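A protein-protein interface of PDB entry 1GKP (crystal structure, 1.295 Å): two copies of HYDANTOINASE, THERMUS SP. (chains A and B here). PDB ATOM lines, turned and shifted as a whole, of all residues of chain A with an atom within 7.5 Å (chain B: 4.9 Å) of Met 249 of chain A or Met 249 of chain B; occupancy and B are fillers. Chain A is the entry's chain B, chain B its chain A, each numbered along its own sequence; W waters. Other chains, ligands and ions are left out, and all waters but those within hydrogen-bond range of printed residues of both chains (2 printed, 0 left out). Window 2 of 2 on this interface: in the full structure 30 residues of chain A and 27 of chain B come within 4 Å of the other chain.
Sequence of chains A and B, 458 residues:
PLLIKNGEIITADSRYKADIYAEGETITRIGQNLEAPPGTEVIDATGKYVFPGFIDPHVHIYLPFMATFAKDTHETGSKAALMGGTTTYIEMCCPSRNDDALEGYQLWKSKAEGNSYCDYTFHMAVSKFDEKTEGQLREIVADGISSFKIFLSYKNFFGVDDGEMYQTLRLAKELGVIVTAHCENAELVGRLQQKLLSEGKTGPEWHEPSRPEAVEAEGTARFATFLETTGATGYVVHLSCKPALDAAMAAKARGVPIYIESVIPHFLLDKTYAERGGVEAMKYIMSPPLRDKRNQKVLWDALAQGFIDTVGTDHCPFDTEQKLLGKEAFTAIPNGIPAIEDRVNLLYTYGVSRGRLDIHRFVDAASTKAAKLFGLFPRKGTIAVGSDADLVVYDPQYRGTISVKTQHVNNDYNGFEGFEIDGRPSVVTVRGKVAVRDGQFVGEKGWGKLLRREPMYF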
ATOM      1  N   THR A 220     -10.808  23.734  19.083  1.00  0.00           N
ATOM      2  CA  THR A 220     -10.304  22.389  19.011  1.00  0.00           C
ATOM      3  C   THR A 220     -11.177  21.597  18.032  1.00  0.00           C
ATOM      4  O   THR A 220     -10.642  20.842  17.206  1.00  0.00           O
ATOM      5  CB  THR A 220     -10.334  21.758  20.433  1.00  0.00           C
ATOM      6  OG1 THR A 220      -9.486  22.538  21.302  1.00  0.00           O
ATOM      7  CG2 THR A 220      -9.774  20.341  20.396  1.00  0.00           C
ATOM      8  N   ALA A 224      -9.949  20.146  14.329  1.00  0.00           N
ATOM      9  CA  ALA A 224     -10.168  18.756  14.014  1.00  0.00           C
ATOM     10  C   ALA A 224     -10.921  18.595  12.694  1.00  0.00           C
ATOM     11  O   ALA A 224     -10.592  17.710  11.911  1.00  0.00           O
ATOM     12  CB  ALA A 224     -10.864  17.997  15.184  1.00  0.00           C
ATOM     13  N   LEU A 239      -3.768  21.432  25.559  1.00  0.00           N
ATOM     14  CA  LEU A 239      -5.182  21.240  25.728  1.00  0.00           C
ATOM     15  C   LEU A 239      -5.440  21.308  27.282  1.00  0.00           C
ATOM     16  O   LEU A 239      -4.789  20.616  28.078  1.00  0.00           O
ATOM     17  CB  LEU A 239      -5.630  19.911  25.161  1.00  0.00           C
ATOM     18  CG  LEU A 239      -7.097  19.619  25.213  1.00  0.00           C
ATOM     19  CD1 LEU A 239      -7.559  18.807  23.996  1.00  0.00           C
ATOM     20  CD2 LEU A 239      -7.469  18.828  26.452  1.00  0.00           C
ATOM     21  N   LYS A 242     -11.932  20.000  29.924  1.00  0.00           N
ATOM     22  CA  LYS A 242     -12.776  18.903  29.500  1.00  0.00           C
ATOM     23  C   LYS A 242     -13.486  19.157  28.161  1.00  0.00           C
ATOM     24  O   LYS A 242     -13.490  18.262  27.345  1.00  0.00           O
ATOM     25  CB  LYS A 242     -13.767  18.462  30.601  1.00  0.00           C
ATOM     26  CG  LYS A 242     -14.533  17.233  30.186  1.00  0.00           C
ATOM     27  CD  LYS A 242     -15.431  16.661  31.274  1.00  0.00           C
ATOM     28  CE  LYS A 242     -16.220  15.446  30.848  1.00  0.00           C
ATOM     29  NZ  LYS A 242     -17.190  15.656  29.785  1.00  0.00           N
ATOM     30  N   PRO A 243     -14.095  20.308  27.950  1.00  0.00           N
ATOM     31  CA  PRO A 243     -14.813  20.430  26.664  1.00  0.00           C
ATOM     32  C   PRO A 243     -13.876  20.361  25.456  1.00  0.00           C
ATOM     33  O   PRO A 243     -14.269  19.835  24.442  1.00  0.00           O
ATOM     34  CB  PRO A 243     -15.494  21.785  26.763  1.00  0.00           C
ATOM     35  CG  PRO A 243     -15.314  22.260  28.031  1.00  0.00           C
ATOM     36  CD  PRO A 243     -14.354  21.458  28.831  1.00  0.00           C
ATOM     37  N   ALA A 244     -12.667  20.857  25.586  1.00  0.00           N
ATOM     38  CA  ALA A 244     -11.687  20.696  24.554  1.00  0.00           C
ATOM     39  C   ALA A 244     -11.288  19.223  24.426  1.00  0.00           C
ATOM     40  O   ALA A 244     -11.142  18.739  23.274  1.00  0.00           O
ATOM     41  CB  ALA A 244     -10.495  21.535  24.763  1.00  0.00           C
ATOM     42  N   LEU A 245     -11.020  18.528  25.524  1.00  0.00           N
ATOM     43  CA  LEU A 245     -10.708  17.116  25.473  1.00  0.00           C
ATOM     44  C   LEU A 245     -11.799  16.340  24.744  1.00  0.00           C
ATOM     45  O   LEU A 245     -11.540  15.497  23.882  1.00  0.00           O
ATOM     46  CB  LEU A 245     -10.465  16.562  26.890  1.00  0.00           C
ATOM     47  CG  LEU A 245     -10.140  15.098  26.899  1.00  0.00           C
ATOM     48  CD1 LEU A 245      -8.807  14.802  26.225  1.00  0.00           C
ATOM     49  CD2 LEU A 245     -10.139  14.622  28.342  1.00  0.00           C
ATOM     50  N   ASP A 246     -13.035  16.639  25.076  1.00  0.00           N
ATOM     51  CA  ASP A 246     -14.163  15.920  24.460  1.00  0.00           C
ATOM     52  C   ASP A 246     -14.173  16.111  22.937  1.00  0.00           C
ATOM     53  O   ASP A 246     -14.384  15.166  22.174  1.00  0.00           O
ATOM     54  CB  ASP A 246     -15.511  16.360  25.028  1.00  0.00           C
ATOM     55  CG  ASP A 246     -15.702  15.954  26.464  1.00  0.00           C
ATOM     56  OD1 ASP A 246     -15.045  15.045  26.943  1.00  0.00           O
ATOM     57  OD2 ASP A 246     -16.583  16.519  27.105  1.00  0.00           O
ATOM     58  N   ALA A 247     -13.892  17.321  22.496  1.00  0.00           N
ATOM     59  CA  ALA A 247     -13.823  17.642  21.035  1.00  0.00           C
ATOM     60  C   ALA A 247     -12.693  16.847  20.365  1.00  0.00           C
ATOM     61  O   ALA A 247     -12.866  16.258  19.299  1.00  0.00           O
ATOM     62  CB  ALA A 247     -13.636  19.134  20.800  1.00  0.00           C
ATOM     63  N   ALA A 248     -11.509  16.890  20.986  1.00  0.00           N
ATOM     64  CA  ALA A 248     -10.352  16.190  20.406  1.00  0.00           C
ATOM     65  C   ALA A 248     -10.567  14.693  20.426  1.00  0.00           C
ATOM     66  O   ALA A 248     -10.219  13.990  19.468  1.00  0.00           O
ATOM     67  CB  ALA A 248      -9.080  16.560  21.097  1.00  0.00           C
ATOM     68  N   MET A 249     -11.140  14.159  21.486  1.00  0.00           N
ATOM     69  CA  MET A 249     -11.403  12.748  21.629  1.00  0.00           C
ATOM     70  C   MET A 249     -12.415  12.263  20.604  1.00  0.00           C
ATOM     71  O   MET A 249     -12.312  11.165  20.092  1.00  0.00           O
ATOM     72  CB  MET A 249     -11.848  12.384  23.026  1.00  0.00           C
ATOM     73  CG  MET A 249     -10.714  12.495  24.019  1.00  0.00           C
ATOM     74  SD  MET A 249      -9.487  11.162  23.848  1.00  0.00           S
ATOM     75  CE  MET A 249     -10.491   9.819  24.319  1.00  0.00           C
ATOM     76  N   ALA A 250     -13.459  13.039  20.396  1.00  0.00           N
ATOM     77  CA  ALA A 250     -14.443  12.644  19.386  1.00  0.00           C
ATOM     78  C   ALA A 250     -13.787  12.549  18.006  1.00  0.00           C
ATOM     79  O   ALA A 250     -14.120  11.627  17.237  1.00  0.00           O
ATOM     80  CB  ALA A 250     -15.597  13.713  19.345  1.00  0.00           C
ATOM     81  N   ALA A 251     -12.871  13.433  17.732  1.00  0.00           N
ATOM     82  CA  ALA A 251     -12.140  13.429  16.448  1.00  0.00           C
ATOM     83  C   ALA A 251     -11.223  12.183  16.382  1.00  0.00           C
ATOM     84  O   ALA A 251     -11.233  11.445  15.395  1.00  0.00           O
ATOM     85  CB  ALA A 251     -11.399  14.633  16.273  1.00  0.00           C
ATOM     86  N   LYS A 252     -10.487  11.897  17.468  1.00  0.00           N
ATOM     87  CA  LYS A 252      -9.677  10.697  17.475  1.00  0.00           C
ATOM     88  C   LYS A 252     -10.550   9.484  17.237  1.00  0.00           C
ATOM     89  O   LYS A 252     -10.188   8.593  16.446  1.00  0.00           O
ATOM     90  CB  LYS A 252      -8.953  10.533  18.852  1.00  0.00           C
ATOM     91  CG  LYS A 252      -7.769  11.406  19.111  1.00  0.00           C
ATOM     92  CD  LYS A 252      -7.019  10.963  20.385  1.00  0.00           C
ATOM     93  CE  LYS A 252      -5.639  11.581  20.461  1.00  0.00           C
ATOM     94  NZ  LYS A 252      -4.839  10.973  21.578  1.00  0.00           N
ATOM     95  N   ALA A 253     -11.718   9.422  17.878  1.00  0.00           N
ATOM     96  CA  ALA A 253     -12.550   8.232  17.851  1.00  0.00           C
ATOM     97  C   ALA A 253     -13.105   7.957  16.436  1.00  0.00           C
ATOM     98  O   ALA A 253     -13.351   6.804  16.094  1.00  0.00           O
ATOM     99  CB  ALA A 253     -13.667   8.244  18.812  1.00  0.00           C
ATOM    100  N   ARG A 254     -13.301   9.027  15.636  1.00  0.00           N
ATOM    101  CA  ARG A 254     -13.865   8.892  14.284  1.00  0.00           C
ATOM    102  C   ARG A 254     -12.750   8.826  13.246  1.00  0.00           C
ATOM    103  O   ARG A 254     -13.018   8.766  12.025  1.00  0.00           O
ATOM    104  CB  ARG A 254     -14.887  10.019  14.030  1.00  0.00           C
ATOM    105  CG  ARG A 254     -14.343  11.337  13.741  1.00  0.00           C
ATOM    106  CD  ARG A 254     -15.434  12.472  13.891  1.00  0.00           C
ATOM    107  NE  ARG A 254     -14.869  13.722  13.454  1.00  0.00           N
ATOM    108  CZ  ARG A 254     -14.735  14.778  14.202  1.00  0.00           C
ATOM    109  NH1 ARG A 254     -15.274  14.786  15.451  1.00  0.00           N
ATOM    110  NH2 ARG A 254     -14.076  15.792  13.707  1.00  0.00           N
ATOM    111  N   GLY A 255     -11.519   8.663  13.669  1.00  0.00           N
ATOM    112  CA  GLY A 255     -10.393   8.439  12.760  1.00  0.00           C
ATOM    113  C   GLY A 255      -9.547   9.554  12.300  1.00  0.00           C
ATOM    114  O   GLY A 255      -8.694   9.311  11.482  1.00  0.00           O
ATOM    115  N   ILE A 258      -5.199  12.999  14.678  1.00  0.00           N
ATOM    116  CA  ILE A 258      -5.028  14.120  15.609  1.00  0.00           C
ATOM    117  C   ILE A 258      -4.478  13.580  16.947  1.00  0.00           C
ATOM    118  O   ILE A 258      -4.885  12.488  17.342  1.00  0.00           O
ATOM    119  CB  ILE A 258      -6.321  14.890  15.806  1.00  0.00           C
ATOM    120  CG1 ILE A 258      -6.104  16.171  16.536  1.00  0.00           C
ATOM    121  CG2 ILE A 258      -7.339  14.057  16.415  1.00  0.00           C
ATOM    122  CD1 ILE A 258      -7.351  17.074  16.649  1.00  0.00           C
ATOM    123  N   ILE A 260      -2.863  14.843  21.004  1.00  0.00           N
ATOM    124  CA  ILE A 260      -3.147  15.778  22.063  1.00  0.00           C
ATOM    125  C   ILE A 260      -1.974  15.927  22.985  1.00  0.00           C
ATOM    126  O   ILE A 260      -1.441  14.951  23.515  1.00  0.00           O
ATOM    127  CB  ILE A 260      -4.344  15.331  22.867  1.00  0.00           C
ATOM    128  CG1 ILE A 260      -5.613  15.268  22.036  1.00  0.00           C
ATOM    129  CG2 ILE A 260      -4.580  16.248  24.076  1.00  0.00           C
ATOM    130  CD1 ILE A 260      -6.693  14.478  22.695  1.00  0.00           C
ATOM    131  N   ALA A 302      -7.088  11.311  31.791  1.00  0.00           N
ATOM    132  CA  ALA A 302      -6.863  11.102  30.350  1.00  0.00           C
ATOM    133  C   ALA A 302      -5.421  10.742  30.091  1.00  0.00           C
ATOM    134  O   ALA A 302      -5.127   9.862  29.269  1.00  0.00           O
ATOM    135  CB  ALA A 302      -7.239  12.333  29.644  1.00  0.00           C
ATOM    136  N   GLN A 305      -4.610   7.014  30.734  1.00  0.00           N
ATOM    137  CA  GLN A 305      -5.154   6.135  29.698  1.00  0.00           C
ATOM    138  C   GLN A 305      -4.525   6.334  28.327  1.00  0.00           C
ATOM    139  O   GLN A 305      -4.897   5.668  27.365  1.00  0.00           O
ATOM    140  CB  GLN A 305      -6.668   6.230  29.616  1.00  0.00           C
ATOM    141  CG  GLN A 305      -7.342   5.611  30.817  1.00  0.00           C
ATOM    142  CD  GLN A 305      -7.399   4.087  30.741  1.00  0.00           C
ATOM    143  OE1 GLN A 305      -6.909   3.465  29.754  1.00  0.00           O
ATOM    144  NE2 GLN A 305      -7.986   3.466  31.766  1.00  0.00           N
ATOM    145  N   GLY A 306      -3.604   7.269  28.222  1.00  0.00           N
ATOM    146  CA  GLY A 306      -2.983   7.574  26.956  1.00  0.00           C
ATOM    147  C   GLY A 306      -3.842   8.385  26.006  1.00  0.00           C
ATOM    148  O   GLY A 306      -3.455   8.549  24.825  1.00  0.00           O
ATOM    149  N   PHE A 307      -4.909   8.978  26.502  1.00  0.00           N
ATOM    150  CA  PHE A 307      -5.744   9.846  25.690  1.00  0.00           C
ATOM    151  C   PHE A 307      -5.020  11.109  25.382  1.00  0.00           C
ATOM    152  O   PHE A 307      -5.158  11.718  24.282  1.00  0.00           O
ATOM    153  CB  PHE A 307      -7.027  10.188  26.399  1.00  0.00           C
ATOM    154  CG  PHE A 307      -7.953   9.039  26.700  1.00  0.00           C
ATOM    155  CD1 PHE A 307      -7.772   7.770  26.167  1.00  0.00           C
ATOM    156  CD2 PHE A 307      -9.023   9.223  27.539  1.00  0.00           C
ATOM    157  CE1 PHE A 307      -8.659   6.762  26.396  1.00  0.00           C
ATOM    158  CE2 PHE A 307      -9.899   8.205  27.817  1.00  0.00           C
ATOM    159  CZ  PHE A 307      -9.748   6.949  27.234  1.00  0.00           C
ATOM    160  N   ILE A 308      -4.259  11.639  26.337  1.00  0.00           N
ATOM    161  CA  ILE A 308      -3.320  12.705  26.104  1.00  0.00           C
ATOM    162  C   ILE A 308      -2.023  12.027  25.749  1.00  0.00           C
ATOM    163  O   ILE A 308      -1.500  11.210  26.516  1.00  0.00           O
ATOM    164  CB  ILE A 308      -3.176  13.604  27.401  1.00  0.00           C
ATOM    165  CG1 ILE A 308      -4.487  14.346  27.629  1.00  0.00           C
ATOM    166  CG2 ILE A 308      -2.032  14.581  27.241  1.00  0.00           C
ATOM    167  CD1 ILE A 308      -4.607  14.956  28.998  1.00  0.00           C
ATOM    168  N   ALA B 244     -20.904  -0.246  23.215  1.00  0.00           N
ATOM    169  CA  ALA B 244     -20.061  -0.744  24.293  1.00  0.00           C
ATOM    170  C   ALA B 244     -18.778   0.051  24.414  1.00  0.00           C
ATOM    171  O   ALA B 244     -18.331   0.373  25.551  1.00  0.00           O
ATOM    172  CB  ALA B 244     -19.730  -2.255  24.024  1.00  0.00           C
ATOM    173  N   LEU B 245     -18.135   0.398  23.336  1.00  0.00           N
ATOM    174  CA  LEU B 245     -16.932   1.152  23.394  1.00  0.00           C
ATOM    175  C   LEU B 245     -17.243   2.497  24.048  1.00  0.00           C
ATOM    176  O   LEU B 245     -16.447   2.983  24.890  1.00  0.00           O
ATOM    177  CB  LEU B 245     -16.361   1.452  21.991  1.00  0.00           C
ATOM    178  CG  LEU B 245     -15.124   2.317  21.883  1.00  0.00           C
ATOM    179  CD1 LEU B 245     -13.915   1.565  22.591  1.00  0.00           C
ATOM    180  CD2 LEU B 245     -14.784   2.644  20.482  1.00  0.00           C
ATOM    181  N   ASP B 246     -18.336   3.170  23.677  1.00  0.00           N
ATOM    182  CA  ASP B 246     -18.724   4.409  24.334  1.00  0.00           C
ATOM    183  C   ASP B 246     -18.858   4.272  25.817  1.00  0.00           C
ATOM    184  O   ASP B 246     -18.369   5.163  26.547  1.00  0.00           O
ATOM    185  CB  ASP B 246     -20.016   4.918  23.697  1.00  0.00           C
ATOM    186  CG  ASP B 246     -19.862   5.427  22.275  1.00  0.00           C
ATOM    187  OD1 ASP B 246     -18.772   5.648  21.812  1.00  0.00           O
ATOM    188  OD2 ASP B 246     -20.887   5.619  21.614  1.00  0.00           O
ATOM    189  N   ALA B 247     -19.451   3.229  26.311  1.00  0.00           N
ATOM    190  CA  ALA B 247     -19.597   3.007  27.739  1.00  0.00           C
ATOM    191  C   ALA B 247     -18.265   2.793  28.430  1.00  0.00           C
ATOM    192  O   ALA B 247     -18.027   3.383  29.498  1.00  0.00           O
ATOM    193  CB  ALA B 247     -20.512   1.840  27.989  1.00  0.00           C
ATOM    194  N   ALA B 248     -17.399   1.978  27.862  1.00  0.00           N
ATOM    195  CA  ALA B 248     -16.111   1.760  28.432  1.00  0.00           C
ATOM    196  C   ALA B 248     -15.247   3.009  28.370  1.00  0.00           C
ATOM    197  O   ALA B 248     -14.498   3.291  29.331  1.00  0.00           O
ATOM    198  CB  ALA B 248     -15.420   0.566  27.746  1.00  0.00           C
ATOM    199  N   MET B 249     -15.297   3.749  27.279  1.00  0.00           N
ATOM    200  CA  MET B 249     -14.534   4.970  27.167  1.00  0.00           C
ATOM    201  C   MET B 249     -14.982   6.042  28.150  1.00  0.00           C
ATOM    202  O   MET B 249     -14.162   6.787  28.666  1.00  0.00           O
ATOM    203  CB  MET B 249     -14.612   5.493  25.743  1.00  0.00           C
ATOM    204  CG  MET B 249     -13.751   4.608  24.795  1.00  0.00           C
ATOM    205  SD  MET B 249     -12.011   4.807  24.981  1.00  0.00           S
ATOM    206  CE  MET B 249     -11.831   6.517  24.407  1.00  0.00           C
ATOM    207  N   ALA B 250     -16.254   6.141  28.370  1.00  0.00           N
ATOM    208  CA  ALA B 250     -16.777   7.125  29.342  1.00  0.00           C
ATOM    209  C   ALA B 250     -16.255   6.766  30.721  1.00  0.00           C
ATOM    210  O   ALA B 250     -15.871   7.659  31.512  1.00  0.00           O
ATOM    211  CB  ALA B 250     -18.321   7.131  29.361  1.00  0.00           C
ATOM    212  N   ALA B 251     -16.186   5.495  31.043  1.00  0.00           N
ATOM    213  CA  ALA B 251     -15.617   5.062  32.301  1.00  0.00           C
ATOM    214  C   ALA B 251     -14.131   5.347  32.355  1.00  0.00           C
ATOM    215  O   ALA B 251     -13.651   5.929  33.339  1.00  0.00           O
ATOM    216  CB  ALA B 251     -15.844   3.624  32.490  1.00  0.00           C
ATOM    217  N   LYS B 252     -13.373   5.073  31.303  1.00  0.00           N
ATOM    218  CA  LYS B 252     -11.986   5.408  31.294  1.00  0.00           C
ATOM    219  C   LYS B 252     -11.823   6.926  31.576  1.00  0.00           C
ATOM    220  O   LYS B 252     -10.923   7.356  32.328  1.00  0.00           O
ATOM    221  CB  LYS B 252     -11.339   5.084  29.951  1.00  0.00           C
ATOM    222  CG  LYS B 252     -11.015   3.597  29.702  1.00  0.00           C
ATOM    223  CD  LYS B 252     -10.065   3.445  28.498  1.00  0.00           C
ATOM    224  CE  LYS B 252      -9.522   2.007  28.425  1.00  0.00           C
ATOM    225  NZ  LYS B 252      -8.508   1.890  27.325  1.00  0.00           N
ATOM    226  N   ALA B 253     -12.566   7.744  30.850  1.00  0.00           N
ATOM    227  CA  ALA B 253     -12.397   9.167  30.926  1.00  0.00           C
ATOM    228  C   ALA B 253     -12.662   9.753  32.297  1.00  0.00           C
ATOM    229  O   ALA B 253     -12.039  10.731  32.670  1.00  0.00           O
ATOM    230  CB  ALA B 253     -13.219   9.856  29.848  1.00  0.00           C
ATOM    231  N   ILE B 260      -9.661  -2.324  27.927  1.00  0.00           N
ATOM    232  CA  ILE B 260     -10.521  -2.852  26.857  1.00  0.00           C
ATOM    233  C   ILE B 260      -9.727  -3.776  25.945  1.00  0.00           C
ATOM    234  O   ILE B 260      -8.706  -3.416  25.436  1.00  0.00           O
ATOM    235  CB  ILE B 260     -11.082  -1.687  26.012  1.00  0.00           C
ATOM    236  CG1 ILE B 260     -11.951  -0.748  26.844  1.00  0.00           C
ATOM    237  CG2 ILE B 260     -11.912  -2.260  24.821  1.00  0.00           C
ATOM    238  CD1 ILE B 260     -12.255   0.568  26.131  1.00  0.00           C
ATOM    239  N   PHE B 307      -7.117   3.297  22.378  1.00  0.00           N
ATOM    240  CA  PHE B 307      -8.338   3.228  23.161  1.00  0.00           C
ATOM    241  C   PHE B 307      -8.708   1.797  23.488  1.00  0.00           C
ATOM    242  O   PHE B 307      -9.257   1.476  24.572  1.00  0.00           O
ATOM    243  CB  PHE B 307      -9.536   3.872  22.443  1.00  0.00           C
ATOM    244  CG  PHE B 307      -9.376   5.342  22.142  1.00  0.00           C
ATOM    245  CD1 PHE B 307      -8.394   6.148  22.724  1.00  0.00           C
ATOM    246  CD2 PHE B 307     -10.270   5.937  21.239  1.00  0.00           C
ATOM    247  CE1 PHE B 307      -8.360   7.476  22.474  1.00  0.00           C
ATOM    248  CE2 PHE B 307     -10.240   7.255  20.980  1.00  0.00           C
ATOM    249  CZ  PHE B 307      -9.289   8.040  21.563  1.00  0.00           C
HETATM  250  O   HOH W   1      -6.777   3.860  26.410  1.00  0.00           O
HETATM  251  O   HOH W   2      -9.398   5.552  33.634  1.00  0.00           O
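OE1 of Gln 305 of chain A lies close to NZ of Lys 252 of chain B (3.3 Å).
The side-chain amino group of Lys 252 of chain B sits at hydrogen-bond distance from the backbone carbonyl oxygen of Phe 307 of chain B, 2.9 Å away.
The side-chain amino group (NZ) of Lys 252 of chain A sits at hydrogen-bond distance from the backbone carbonyl oxygen (O) of Phe 307 of chain A (2.8 Å).
N of Phe 307 of chain A lies within hydrogen-bond range of O of Ala 302 of chain A (2.9 Å).
Met 249 of chain A touches Met 249 of chain B.
CE of Met 249 of chain A touches CZ of Phe 307 of chain B (3.5 Å).
Phe 307 of chain B touches Lys 252 of chain A (CZ to CB, 3.7 Å).
Phe 307 of chain A touches Met 249 of chain B.
Phe 307 of chain A touches Lys 252 of chain B.
Phe 307 of chain B touches Phe 307 of chain A (CD1 to CE1, 3.7 Å).
Of chain B, only Met 249 and Phe 307 come within 4 Å of Met 249 of chain A.
Of the printed residues of chain B, Gln 305 of chain A touches Lys 252 (3.3 Å).
No residue of chain A comes within 4 Å of Ala 248 of chain B.
Of the printed residues of chain A, Lys 252 of chain B touches Gln 305 and Phe 307.
The nearest printed residue of chain B that does not touch Met 249 of chain A is Ala 253 of chain B (6.2 Å).
The nearest printed residue of chain A that does not touch Phe 307 of chain B is Ala 253 of chain A (4.01 Å).
Hydrophobic or aromatic side chains of chain B that line the printed part of chain A: Met 249 and Phe 307.
Of the 24 printed residues of chain A, 4 touch a printed residue of chain B.
Hydrophobic or aromatic side chains of chain A that line the printed part of chain B: Met 249 and Phe 307.
Among the printed residues, no Asp or Glu carboxylate lies within 4 Å of a Lys or Arg side-chain nitrogen of the other chain.
Met 249 of chain B touches its own counterpart, Met 249 of chain A.
Met 249 of chain A touches Phe 307 of chain B, and with the chains exchanged Phe 307 of chain A touches Met 249 of chain B.
Lys 252 of chain A touches Phe 307 of chain B, and with the chains exchanged Phe 307 of chain A touches Lys 252 of chain B.
Phe 307 of chain B touches its own counterpart, Phe 307 of chain A.
Of the 7 pairs that touch across the chains among the printed residues, 6 have their exchanged pair printed and touching as well.
Water W2 lies within hydrogen-bond range of the backbone carbonyl oxygen of Lys 252 of chain B (2.7 Å) and the side-chain amide nitrogen of Gln 305 of chain A (3.1 Å).
Water W1 lies within hydrogen-bond range of O of Gln 305 of chain A (2.8 Å) and NZ of Lys 252 of chain B (2.8 Å).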
